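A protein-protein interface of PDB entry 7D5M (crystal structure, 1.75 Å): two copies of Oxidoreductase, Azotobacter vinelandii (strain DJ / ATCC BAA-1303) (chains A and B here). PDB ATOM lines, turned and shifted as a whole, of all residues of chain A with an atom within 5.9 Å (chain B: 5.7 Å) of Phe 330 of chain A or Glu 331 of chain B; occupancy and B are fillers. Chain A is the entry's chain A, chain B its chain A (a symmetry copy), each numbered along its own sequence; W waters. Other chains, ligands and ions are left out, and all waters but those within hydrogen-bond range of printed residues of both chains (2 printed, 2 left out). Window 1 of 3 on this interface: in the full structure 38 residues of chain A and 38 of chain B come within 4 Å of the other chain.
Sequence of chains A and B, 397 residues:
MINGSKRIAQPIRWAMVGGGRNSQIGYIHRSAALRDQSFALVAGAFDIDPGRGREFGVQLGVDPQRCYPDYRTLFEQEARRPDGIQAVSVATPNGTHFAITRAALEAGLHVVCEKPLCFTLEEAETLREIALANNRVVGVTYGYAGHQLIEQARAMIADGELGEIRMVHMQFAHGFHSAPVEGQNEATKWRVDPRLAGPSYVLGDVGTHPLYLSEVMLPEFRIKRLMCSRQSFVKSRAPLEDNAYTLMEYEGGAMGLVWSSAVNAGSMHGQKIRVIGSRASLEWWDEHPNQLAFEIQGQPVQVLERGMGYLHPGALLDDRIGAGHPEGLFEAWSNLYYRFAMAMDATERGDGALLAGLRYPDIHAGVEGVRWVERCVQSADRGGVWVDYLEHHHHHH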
ATOM      1  N   TYR A  27     -25.045 -17.238  35.958  1.00  0.00           N
ATOM      2  CA  TYR A  27     -24.129 -16.966  34.825  1.00  0.00           C
ATOM      3  C   TYR A  27     -23.817 -15.467  34.710  1.00  0.00           C
ATOM      4  O   TYR A  27     -22.641 -15.104  34.522  1.00  0.00           O
ATOM      5  CB  TYR A  27     -24.673 -17.501  33.502  1.00  0.00           C
ATOM      6  CG  TYR A  27     -23.740 -17.153  32.376  1.00  0.00           C
ATOM      7  CD1 TYR A  27     -22.476 -17.716  32.318  1.00  0.00           C
ATOM      8  CD2 TYR A  27     -24.061 -16.170  31.456  1.00  0.00           C
ATOM      9  CE1 TYR A  27     -21.576 -17.363  31.331  1.00  0.00           C
ATOM     10  CE2 TYR A  27     -23.172 -15.814  30.455  1.00  0.00           C
ATOM     11  CZ  TYR A  27     -21.926 -16.407  30.394  1.00  0.00           C
ATOM     12  OH  TYR A  27     -21.037 -16.053  29.422  1.00  0.00           O
ATOM     13  N   ILE A  28     -24.818 -14.598  34.775  1.00  0.00           N
ATOM     14  CA  ILE A  28     -24.562 -13.144  34.565  1.00  0.00           C
ATOM     15  C   ILE A  28     -23.656 -12.618  35.688  1.00  0.00           C
ATOM     16  O   ILE A  28     -22.789 -11.775  35.398  1.00  0.00           O
ATOM     17  CB  ILE A  28     -25.848 -12.318  34.380  1.00  0.00           C
ATOM     18  CG1 ILE A  28     -25.488 -10.886  33.969  1.00  0.00           C
ATOM     19  CG2 ILE A  28     -26.743 -12.348  35.613  1.00  0.00           C
ATOM     20  CD1 ILE A  28     -26.620 -10.135  33.327  1.00  0.00           C
ATOM     21  N   SER A  31     -20.214 -13.774  34.390  1.00  0.00           N
ATOM     22  CA  SER A  31     -19.903 -13.045  33.136  1.00  0.00           C
ATOM     23  C   SER A  31     -19.385 -11.645  33.486  1.00  0.00           C
ATOM     24  O   SER A  31     -18.341 -11.236  32.955  1.00  0.00           O
ATOM     25  CB  SER A  31     -21.096 -13.021  32.222  1.00  0.00           C
ATOM     26  OG  SER A  31     -20.708 -12.609  30.919  1.00  0.00           O
ATOM     27  N   ALA A  32     -20.076 -10.942  34.381  1.00  0.00           N
ATOM     28  CA  ALA A  32     -19.763  -9.551  34.773  1.00  0.00           C
ATOM     29  C   ALA A  32     -18.523  -9.514  35.680  1.00  0.00           C
ATOM     30  O   ALA A  32     -17.691  -8.611  35.503  1.00  0.00           O
ATOM     31  CB  ALA A  32     -20.961  -8.937  35.459  1.00  0.00           C
ATOM     32  N   ARG A  35     -15.038 -10.442  33.931  1.00  0.00           N
ATOM     33  CA  ARG A  35     -14.702  -9.530  32.820  1.00  0.00           C
ATOM     34  C   ARG A  35     -13.638  -8.528  33.272  1.00  0.00           C
ATOM     35  O   ARG A  35     -13.701  -8.045  34.429  1.00  0.00           O
ATOM     36  CB  ARG A  35     -15.958  -8.814  32.337  1.00  0.00           C
ATOM     37  CG  ARG A  35     -15.806  -8.220  30.947  1.00  0.00           C
ATOM     38  CD  ARG A  35     -17.124  -7.594  30.560  1.00  0.00           C
ATOM     39  NE  ARG A  35     -17.204  -7.275  29.149  1.00  0.00           N
ATOM     40  CZ  ARG A  35     -18.315  -6.886  28.538  1.00  0.00           C
ATOM     41  NH1 ARG A  35     -19.419  -6.701  29.239  1.00  0.00           N
ATOM     42  NH2 ARG A  35     -18.298  -6.611  27.246  1.00  0.00           N
ATOM     43  N   HIS A 147     -26.537   0.594  33.154  1.00  0.00           N
ATOM     44  CA  HIS A 147     -26.709   1.167  31.792  1.00  0.00           C
ATOM     45  C   HIS A 147     -26.324   2.651  31.810  1.00  0.00           C
ATOM     46  O   HIS A 147     -26.876   3.397  32.653  1.00  0.00           O
ATOM     47  CB  HIS A 147     -28.123   0.934  31.263  1.00  0.00           C
ATOM     48  CG  HIS A 147     -28.323  -0.452  30.747  1.00  0.00           C
ATOM     49  ND1 HIS A 147     -29.206  -1.342  31.332  1.00  0.00           N
ATOM     50  CD2 HIS A 147     -27.752  -1.112  29.715  1.00  0.00           C
ATOM     51  CE1 HIS A 147     -29.163  -2.487  30.678  1.00  0.00           C
ATOM     52  NE2 HIS A 147     -28.293  -2.371  29.690  1.00  0.00           N
ATOM     53  N   GLY A 328     -25.800  -4.474  25.986  1.00  0.00           N
ATOM     54  CA  GLY A 328     -26.946  -5.140  26.626  1.00  0.00           C
ATOM     55  C   GLY A 328     -26.778  -5.225  28.125  1.00  0.00           C
ATOM     56  O   GLY A 328     -25.894  -4.553  28.685  1.00  0.00           O
ATOM     57  N   LEU A 329     -27.601  -6.037  28.767  1.00  0.00           N
ATOM     58  CA  LEU A 329     -27.636  -6.102  30.247  1.00  0.00           C
ATOM     59  C   LEU A 329     -26.308  -6.659  30.785  1.00  0.00           C
ATOM     60  O   LEU A 329     -25.971  -6.347  31.931  1.00  0.00           O
ATOM     61  CB  LEU A 329     -28.834  -6.953  30.678  1.00  0.00           C
ATOM     62  CG  LEU A 329     -29.069  -7.052  32.190  1.00  0.00           C
ATOM     63  CD1 LEU A 329     -29.318  -5.687  32.802  1.00  0.00           C
ATOM     64  CD2 LEU A 329     -30.249  -7.970  32.487  1.00  0.00           C
ATOM     65  N   PHE A 330     -25.552  -7.434  30.006  1.00  0.00           N
ATOM     66  CA  PHE A 330     -24.240  -7.956  30.481  1.00  0.00           C
ATOM     67  C   PHE A 330     -23.263  -6.792  30.690  1.00  0.00           C
ATOM     68  O   PHE A 330     -22.476  -6.830  31.656  1.00  0.00           O
ATOM     69  CB  PHE A 330     -23.687  -9.048  29.566  1.00  0.00           C
ATOM     70  CG  PHE A 330     -24.428 -10.351  29.715  1.00  0.00           C
ATOM     71  CD1 PHE A 330     -24.040 -11.290  30.656  1.00  0.00           C
ATOM     72  CD2 PHE A 330     -25.537 -10.625  28.924  1.00  0.00           C
ATOM     73  CE1 PHE A 330     -24.731 -12.487  30.793  1.00  0.00           C
ATOM     74  CE2 PHE A 330     -26.230 -11.819  29.070  1.00  0.00           C
ATOM     75  CZ  PHE A 330     -25.831 -12.740  30.014  1.00  0.00           C
ATOM     76  N   GLU A 331     -23.331  -5.771  29.843  1.00  0.00           N
ATOM     77  CA  GLU A 331     -22.472  -4.568  29.996  1.00  0.00           C
ATOM     78  C   GLU A 331     -22.885  -3.826  31.271  1.00  0.00           C
ATOM     79  O   GLU A 331     -22.001  -3.437  32.043  1.00  0.00           O
ATOM     80  CB  GLU A 331     -22.558  -3.666  28.767  1.00  0.00           C
ATOM     81  CG  GLU A 331     -21.701  -4.170  27.623  1.00  0.00           C
ATOM     82  CD  GLU A 331     -22.119  -5.514  27.052  1.00  0.00           C
ATOM     83  OE1 GLU A 331     -21.345  -6.502  27.214  1.00  0.00           O
ATOM     84  OE2 GLU A 331     -23.217  -5.587  26.473  1.00  0.00           O
ATOM     85  N   ALA A 332     -24.184  -3.623  31.469  1.00  0.00           N
ATOM     86  CA  ALA A 332     -24.728  -2.968  32.682  1.00  0.00           C
ATOM     87  C   ALA A 332     -24.181  -3.699  33.919  1.00  0.00           C
ATOM     88  O   ALA A 332     -23.657  -3.043  34.849  1.00  0.00           O
ATOM     89  CB  ALA A 332     -26.235  -2.969  32.652  1.00  0.00           C
ATOM     90  N   TRP A 333     -24.282  -5.024  33.947  1.00  0.00           N
ATOM     91  CA  TRP A 333     -23.804  -5.803  35.121  1.00  0.00           C
ATOM     92  C   TRP A 333     -22.283  -5.694  35.258  1.00  0.00           C
ATOM     93  O   TRP A 333     -21.799  -5.635  36.409  1.00  0.00           O
ATOM     94  CB  TRP A 333     -24.230  -7.260  35.035  1.00  0.00           C
ATOM     95  CG  TRP A 333     -25.616  -7.508  35.518  1.00  0.00           C
ATOM     96  CD1 TRP A 333     -26.791  -7.006  35.035  1.00  0.00           C
ATOM     97  CD2 TRP A 333     -25.959  -8.383  36.600  1.00  0.00           C
ATOM     98  NE1 TRP A 333     -27.843  -7.507  35.753  1.00  0.00           N
ATOM     99  CE2 TRP A 333     -27.362  -8.356  36.715  1.00  0.00           C
ATOM    100  CE3 TRP A 333     -25.210  -9.173  37.481  1.00  0.00           C
ATOM    101  CZ2 TRP A 333     -28.035  -9.093  37.690  1.00  0.00           C
ATOM    102  CZ3 TRP A 333     -25.878  -9.907  38.435  1.00  0.00           C
ATOM    103  CH2 TRP A 333     -27.273  -9.851  38.544  1.00  0.00           C
ATOM    104  N   SER A 334     -21.561  -5.711  34.140  1.00  0.00           N
ATOM    105  CA  SER A 334     -20.080  -5.551  34.119  1.00  0.00           C
ATOM    106  C   SER A 334     -19.695  -4.179  34.686  1.00  0.00           C
ATOM    107  O   SER A 334     -18.679  -4.096  35.403  1.00  0.00           O
ATOM    108  CB  SER A 334     -19.510  -5.757  32.746  1.00  0.00           C
ATOM    109  OG  SER A 334     -19.820  -7.058  32.266  1.00  0.00           O
ATOM    110  N   ASN A 335     -20.479  -3.146  34.382  1.00  0.00           N
ATOM    111  CA  ASN A 335     -20.251  -1.764  34.867  1.00  0.00           C
ATOM    112  C   ASN A 335     -20.420  -1.712  36.392  1.00  0.00           C
ATOM    113  O   ASN A 335     -19.652  -0.993  37.038  1.00  0.00           O
ATOM    114  CB  ASN A 335     -21.154  -0.777  34.128  1.00  0.00           C
ATOM    115  CG  ASN A 335     -20.793  -0.705  32.664  1.00  0.00           C
ATOM    116  OD1 ASN A 335     -19.651  -0.995  32.305  1.00  0.00           O
ATOM    117  ND2 ASN A 335     -21.748  -0.320  31.824  1.00  0.00           N
ATOM    118  N   ARG B  35     -14.107 -14.859  27.325  1.00  0.00           N
ATOM    119  CA  ARG B  35     -15.371 -15.268  27.969  1.00  0.00           C
ATOM    120  C   ARG B  35     -15.467 -16.795  28.004  1.00  0.00           C
ATOM    121  O   ARG B  35     -15.071 -17.459  27.014  1.00  0.00           O
ATOM    122  CB  ARG B  35     -16.554 -14.663  27.224  1.00  0.00           C
ATOM    123  CG  ARG B  35     -17.830 -14.647  28.048  1.00  0.00           C
ATOM    124  CD  ARG B  35     -18.907 -13.976  27.231  1.00  0.00           C
ATOM    125  NE  ARG B  35     -20.072 -13.620  28.016  1.00  0.00           N
ATOM    126  CZ  ARG B  35     -21.067 -12.868  27.567  1.00  0.00           C
ATOM    127  NH1 ARG B  35     -21.065 -12.457  26.312  1.00  0.00           N
ATOM    128  NH2 ARG B  35     -22.096 -12.595  28.350  1.00  0.00           N
ATOM    129  N   GLY B 146     -23.444 -13.862  14.940  1.00  0.00           N
ATOM    130  CA  GLY B 146     -23.533 -14.498  16.261  1.00  0.00           C
ATOM    131  C   GLY B 146     -24.880 -14.310  16.938  1.00  0.00           C
ATOM    132  O   GLY B 146     -25.138 -15.000  17.950  1.00  0.00           O
ATOM    133  N   GLN B 148     -28.563 -14.895  17.849  1.00  0.00           N
ATOM    134  CA  GLN B 148     -29.434 -16.102  17.785  1.00  0.00           C
ATOM    135  C   GLN B 148     -30.471 -15.971  16.665  1.00  0.00           C
ATOM    136  O   GLN B 148     -30.782 -16.990  16.015  1.00  0.00           O
ATOM    137  CB  GLN B 148     -30.171 -16.320  19.108  1.00  0.00           C
ATOM    138  CG  GLN B 148     -29.285 -16.804  20.256  1.00  0.00           C
ATOM    139  CD  GLN B 148     -28.600 -15.701  21.030  1.00  0.00           C
ATOM    140  OE1 GLN B 148     -27.770 -14.961  20.500  1.00  0.00           O
ATOM    141  NE2 GLN B 148     -28.888 -15.626  22.318  1.00  0.00           N
ATOM    142  N   ARG B 320     -27.848 -16.741  27.010  1.00  0.00           N
ATOM    143  CA  ARG B 320     -27.034 -16.600  28.249  1.00  0.00           C
ATOM    144  C   ARG B 320     -27.901 -16.065  29.388  1.00  0.00           C
ATOM    145  O   ARG B 320     -27.485 -16.157  30.554  1.00  0.00           O
ATOM    146  CB  ARG B 320     -25.843 -15.678  27.985  1.00  0.00           C
ATOM    147  CG  ARG B 320     -24.862 -16.249  26.972  1.00  0.00           C
ATOM    148  CD  ARG B 320     -24.027 -15.190  26.279  1.00  0.00           C
ATOM    149  NE  ARG B 320     -23.253 -15.792  25.209  1.00  0.00           N
ATOM    150  CZ  ARG B 320     -22.064 -16.375  25.355  1.00  0.00           C
ATOM    151  NH1 ARG B 320     -21.462 -16.391  26.534  1.00  0.00           N
ATOM    152  NH2 ARG B 320     -21.459 -16.913  24.313  1.00  0.00           N
ATOM    153  N   ILE B 321     -29.081 -15.539  29.061  1.00  0.00           N
ATOM    154  CA  ILE B 321     -30.078 -15.105  30.071  1.00  0.00           C
ATOM    155  C   ILE B 321     -31.474 -15.208  29.447  1.00  0.00           C
ATOM    156  O   ILE B 321     -31.577 -15.241  28.215  1.00  0.00           O
ATOM    157  CB  ILE B 321     -29.731 -13.692  30.577  1.00  0.00           C
ATOM    158  CG1 ILE B 321     -30.502 -13.340  31.854  1.00  0.00           C
ATOM    159  CG2 ILE B 321     -29.914 -12.681  29.454  1.00  0.00           C
ATOM    160  CD1 ILE B 321     -29.955 -12.164  32.623  1.00  0.00           C
ATOM    161  N   PRO B 326     -32.140  -7.836  27.494  1.00  0.00           N
ATOM    162  CA  PRO B 326     -31.482  -7.583  26.214  1.00  0.00           C
ATOM    163  C   PRO B 326     -30.034  -8.081  26.187  1.00  0.00           C
ATOM    164  O   PRO B 326     -29.235  -7.645  26.999  1.00  0.00           O
ATOM    165  CB  PRO B 326     -31.498  -6.055  26.075  1.00  0.00           C
ATOM    166  CG  PRO B 326     -31.541  -5.565  27.500  1.00  0.00           C
ATOM    167  CD  PRO B 326     -32.346  -6.598  28.265  1.00  0.00           C
ATOM    168  N   GLU B 327     -29.743  -9.000  25.264  1.00  0.00           N
ATOM    169  CA  GLU B 327     -28.350  -9.314  24.874  1.00  0.00           C
ATOM    170  C   GLU B 327     -27.908  -8.277  23.833  1.00  0.00           C
ATOM    171  O   GLU B 327     -28.760  -7.496  23.322  1.00  0.00           O
ATOM    172  CB  GLU B 327     -28.249 -10.757  24.388  1.00  0.00           C
ATOM    173  CG  GLU B 327     -28.445 -11.752  25.519  1.00  0.00           C
ATOM    174  CD  GLU B 327     -28.158 -13.203  25.178  1.00  0.00           C
ATOM    175  OE1 GLU B 327     -27.729 -13.485  24.037  1.00  0.00           O
ATOM    176  OE2 GLU B 327     -28.339 -14.047  26.087  1.00  0.00           O
ATOM    177  N   GLY B 328     -26.611  -8.221  23.563  1.00  0.00           N
ATOM    178  CA  GLY B 328     -26.064  -7.230  22.622  1.00  0.00           C
ATOM    179  C   GLY B 328     -24.980  -7.823  21.753  1.00  0.00           C
ATOM    180  O   GLY B 328     -24.827  -9.057  21.714  1.00  0.00           O
ATOM    181  N   LEU B 329     -24.234  -6.969  21.072  1.00  0.00           N
ATOM    182  CA  LEU B 329     -23.236  -7.426  20.077  1.00  0.00           C
ATOM    183  C   LEU B 329     -22.107  -8.201  20.775  1.00  0.00           C
ATOM    184  O   LEU B 329     -21.481  -9.034  20.114  1.00  0.00           O
ATOM    185  CB  LEU B 329     -22.711  -6.211  19.308  1.00  0.00           C
ATOM    186  CG  LEU B 329     -21.727  -6.518  18.172  1.00  0.00           C
ATOM    187  CD1 LEU B 329     -22.358  -7.406  17.117  1.00  0.00           C
ATOM    188  CD2 LEU B 329     -21.236  -5.227  17.528  1.00  0.00           C
ATOM    189  N   PHE B 330     -21.849  -7.975  22.064  1.00  0.00           N
ATOM    190  CA  PHE B 330     -20.790  -8.738  22.782  1.00  0.00           C
ATOM    191  C   PHE B 330     -21.183 -10.218  22.866  1.00  0.00           C
ATOM    192  O   PHE B 330     -20.297 -11.086  22.742  1.00  0.00           O
ATOM    193  CB  PHE B 330     -20.458  -8.125  24.142  1.00  0.00           C
ATOM    194  CG  PHE B 330     -19.665  -6.850  24.019  1.00  0.00           C
ATOM    195  CD1 PHE B 330     -18.282  -6.872  23.969  1.00  0.00           C
ATOM    196  CD2 PHE B 330     -20.313  -5.625  23.926  1.00  0.00           C
ATOM    197  CE1 PHE B 330     -17.557  -5.693  23.850  1.00  0.00           C
ATOM    198  CE2 PHE B 330     -19.584  -4.449  23.798  1.00  0.00           C
ATOM    199  CZ  PHE B 330     -18.208  -4.490  23.748  1.00  0.00           C
ATOM    200  N   GLU B 331     -22.470 -10.505  23.032  1.00  0.00           N
ATOM    201  CA  GLU B 331     -22.961 -11.907  23.064  1.00  0.00           C
ATOM    202  C   GLU B 331     -22.772 -12.528  21.676  1.00  0.00           C
ATOM    203  O   GLU B 331     -22.284 -13.660  21.595  1.00  0.00           O
ATOM    204  CB  GLU B 331     -24.418 -11.974  23.517  1.00  0.00           C
ATOM    205  CG  GLU B 331     -24.558 -11.858  25.022  1.00  0.00           C
ATOM    206  CD  GLU B 331     -24.111 -10.530  25.608  1.00  0.00           C
ATOM    207  OE1 GLU B 331     -23.087 -10.517  26.351  1.00  0.00           O
ATOM    208  OE2 GLU B 331     -24.757  -9.512  25.308  1.00  0.00           O
ATOM    209  N   ALA B 332     -23.166 -11.813  20.626  1.00  0.00           N
ATOM    210  CA  ALA B 332     -22.996 -12.266  19.225  1.00  0.00           C
ATOM    211  C   ALA B 332     -21.518 -12.632  19.008  1.00  0.00           C
ATOM    212  O   ALA B 332     -21.220 -13.734  18.491  1.00  0.00           O
ATOM    213  CB  ALA B 332     -23.456 -11.199  18.265  1.00  0.00           C
ATOM    214  N   TRP B 333     -20.601 -11.749  19.390  1.00  0.00           N
ATOM    215  CA  TRP B 333     -19.152 -12.015  19.186  1.00  0.00           C
ATOM    216  C   TRP B 333     -18.694 -13.196  20.044  1.00  0.00           C
ATOM    217  O   TRP B 333     -17.844 -13.978  19.565  1.00  0.00           O
ATOM    218  CB  TRP B 333     -18.312 -10.782  19.480  1.00  0.00           C
ATOM    219  CG  TRP B 333     -18.230  -9.827  18.341  1.00  0.00           C
ATOM    220  CD1 TRP B 333     -19.241  -9.145  17.724  1.00  0.00           C
ATOM    221  CD2 TRP B 333     -17.014  -9.426  17.698  1.00  0.00           C
ATOM    222  NE1 TRP B 333     -18.730  -8.350  16.733  1.00  0.00           N
ATOM    223  CE2 TRP B 333     -17.369  -8.500  16.698  1.00  0.00           C
ATOM    224  CE3 TRP B 333     -15.667  -9.770  17.872  1.00  0.00           C
ATOM    225  CZ2 TRP B 333     -16.415  -7.915  15.865  1.00  0.00           C
ATOM    226  CZ3 TRP B 333     -14.728  -9.184  17.054  1.00  0.00           C
ATOM    227  CH2 TRP B 333     -15.105  -8.280  16.053  1.00  0.00           C
ATOM    228  N   SER B 334     -19.197 -13.297  21.273  1.00  0.00           N
ATOM    229  CA  SER B 334     -18.889 -14.427  22.194  1.00  0.00           C
ATOM    230  C   SER B 334     -19.369 -15.748  21.579  1.00  0.00           C
ATOM    231  O   SER B 334     -18.663 -16.764  21.728  1.00  0.00           O
ATOM    232  CB  SER B 334     -19.472 -14.215  23.560  1.00  0.00           C
ATOM    233  OG  SER B 334     -18.963 -13.022  24.141  1.00  0.00           O
ATOM    234  N   ASN B 335     -20.521 -15.732  20.909  1.00  0.00           N
ATOM    235  CA  ASN B 335     -21.106 -16.920  20.244  1.00  0.00           C
ATOM    236  C   ASN B 335     -20.200 -17.371  19.090  1.00  0.00           C
ATOM    237  O   ASN B 335     -20.058 -18.583  18.901  1.00  0.00           O
ATOM    238  CB  ASN B 335     -22.543 -16.640  19.806  1.00  0.00           C
ATOM    239  CG  ASN B 335     -23.441 -16.421  21.000  1.00  0.00           C
ATOM    240  OD1 ASN B 335     -23.136 -16.915  22.087  1.00  0.00           O
ATOM    241  ND2 ASN B 335     -24.536 -15.695  20.808  1.00  0.00           N
ATOM    242  N   LEU B 336     -19.576 -16.451  18.355  1.00  0.00           N
ATOM    243  CA  LEU B 336     -18.607 -16.846  17.302  1.00  0.00           C
ATOM    244  C   LEU B 336     -17.340 -17.391  17.963  1.00  0.00           C
ATOM    245  O   LEU B 336     -16.849 -18.435  17.515  1.00  0.00           O
ATOM    246  CB  LEU B 336     -18.242 -15.656  16.415  1.00  0.00           C
ATOM    247  CG  LEU B 336     -19.365 -15.056  15.573  1.00  0.00           C
ATOM    248  CD1 LEU B 336     -18.746 -14.267  14.437  1.00  0.00           C
ATOM    249  CD2 LEU B 336     -20.339 -16.099  15.054  1.00  0.00           C
HETATM  250  O   HOH W   1     -20.946  -9.197  27.421  1.00  0.00           O
HETATM  251  O   HOH W   2     -27.607 -15.543  33.889  1.00  0.00           O
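O of Pro 326 of chain B lies within hydrogen-bond range of N of Leu 329 of chain A (2.9 Å).
OG of Ser 31 of chain A is in hydrogen-bond range of NH2 of Arg 35 of chain B, at 2.9 Å.
The guanidinium group (NE) of Arg 35 of chain B sits at hydrogen-bond distance from the side-chain hydroxyl (OH) of Tyr 27 of chain A, 3.0 Å away.
OH of Tyr 27 of chain A sits at hydrogen-bond distance from NH1 of Arg 320 of chain B, at 2.9 Å.
O of Glu 331 of chain B lies close to ND2 of Asn 335 of chain B, at 3.1 Å.
The side-chain carboxylate of Glu 327 of chain B sits at hydrogen-bond distance from the backbone NH of Arg 320 of chain B (2.9 Å).
NH1 of Arg 35 of chain B lies within salt-bridge range of OE1 of Glu 331 of chain B (2.8 Å).
A ring nitrogen (NE2) of His 147 of chain A is in hydrogen-bond range of the backbone carbonyl oxygen (O) of Gly 328 of chain A (3.4 Å).
The backbone carbonyl oxygen of Glu 331 of chain A lies close to the side-chain amide nitrogen of Asn 335 of chain A (3.1 Å).
The side-chain carboxylate of Glu 331 of chain A lies within salt-bridge range of the guanidinium group of Arg 35 of chain A, at 2.8 Å.
Among the printed residues, merely in contact across the chains: Phe 330 of chain A with Arg 35 of chain B (3.3 Å), Arg 35 of chain A with Phe 330 of chain B (3.3 Å), Gly 328 of chain A with Pro 326 of chain B (3.4 Å), Phe 330 of chain A with Glu 331 of chain B (3.6 Å), Glu 331 of chain A with Phe 330 of chain B (3.6 Å), Phe 330 of chain A with Arg 320 of chain B (3.6 Å), Phe 330 of chain A with Ile 321 of chain B (3.8 Å) and Ile 28 of chain A with Ile 321 of chain B (3.97 Å).
Of chain A, only Phe 330 (3.6 Å) comes within 4 Å of Glu 331 of chain B.
Printed residues of chain B within 4 Å of Ile 28 of chain A: Ile 321 (3.97 Å).
Of the printed residues of chain A, Pro 326 of chain B touches Gly 328 and Leu 329.
Printed residues of chain A within 4 Å of Arg 35 of chain B: Tyr 27 (3.0 Å), Ser 31 (2.9 Å) and Phe 330 (3.3 Å).
Ala 32 of chain A touches none of the printed residues of chain B.
Asn 335 of chain A touches none of the printed residues of chain B.
The nearest residue of chain A that does not touch Glu 331 of chain B is Glu 331 of chain A (4.4 Å).
Hydrophobic or aromatic side chains of chain B that line the printed part of chain A: Ile 321 and Phe 330.
Printed residues of chain A that touch a printed residue of chain B: Tyr 27, Ile 28, Ser 31, Arg 35, Gly 328, Leu 329, Phe 330 and Glu 331.
Hydrophobic or aromatic side chains of chain A that line the printed part of chain B: Tyr 27, Ile 28, Leu 329 and Phe 330.
Among the printed residues, 12 pairs touch across the chains.
Among the printed residues, no Asp or Glu carboxylate lies within 4 Å of a Lys or Arg side-chain nitrogen of the other chain.
Arg 35 of chain A touches Phe 330 of chain B, and with the chains exchanged Phe 330 of chain A touches Arg 35 of chain B.
Phe 330 of chain A touches Glu 331 of chain B, and with the chains exchanged Glu 331 of chain A touches Phe 330 of chain B.
Positions printed for both chains: 35, 328, 329, 330, 331, 332, 333, 334 and 335.
Water W1 lies within hydrogen-bond range of OE1 of Glu 331 of chain A (2.7 Å), OE1 of Glu 331 of chain B (2.7 Å), NH1 of Arg 35 of chain A (3.4 Å) and NH1 of Arg 35 of chain B (3.4 Å).
Water W2 bridges the backbone NH (N) of Ile 28 of chain A (3.1 Å) and the backbone carbonyl oxygen (O) of Arg 320 of chain B (3.4 Å).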
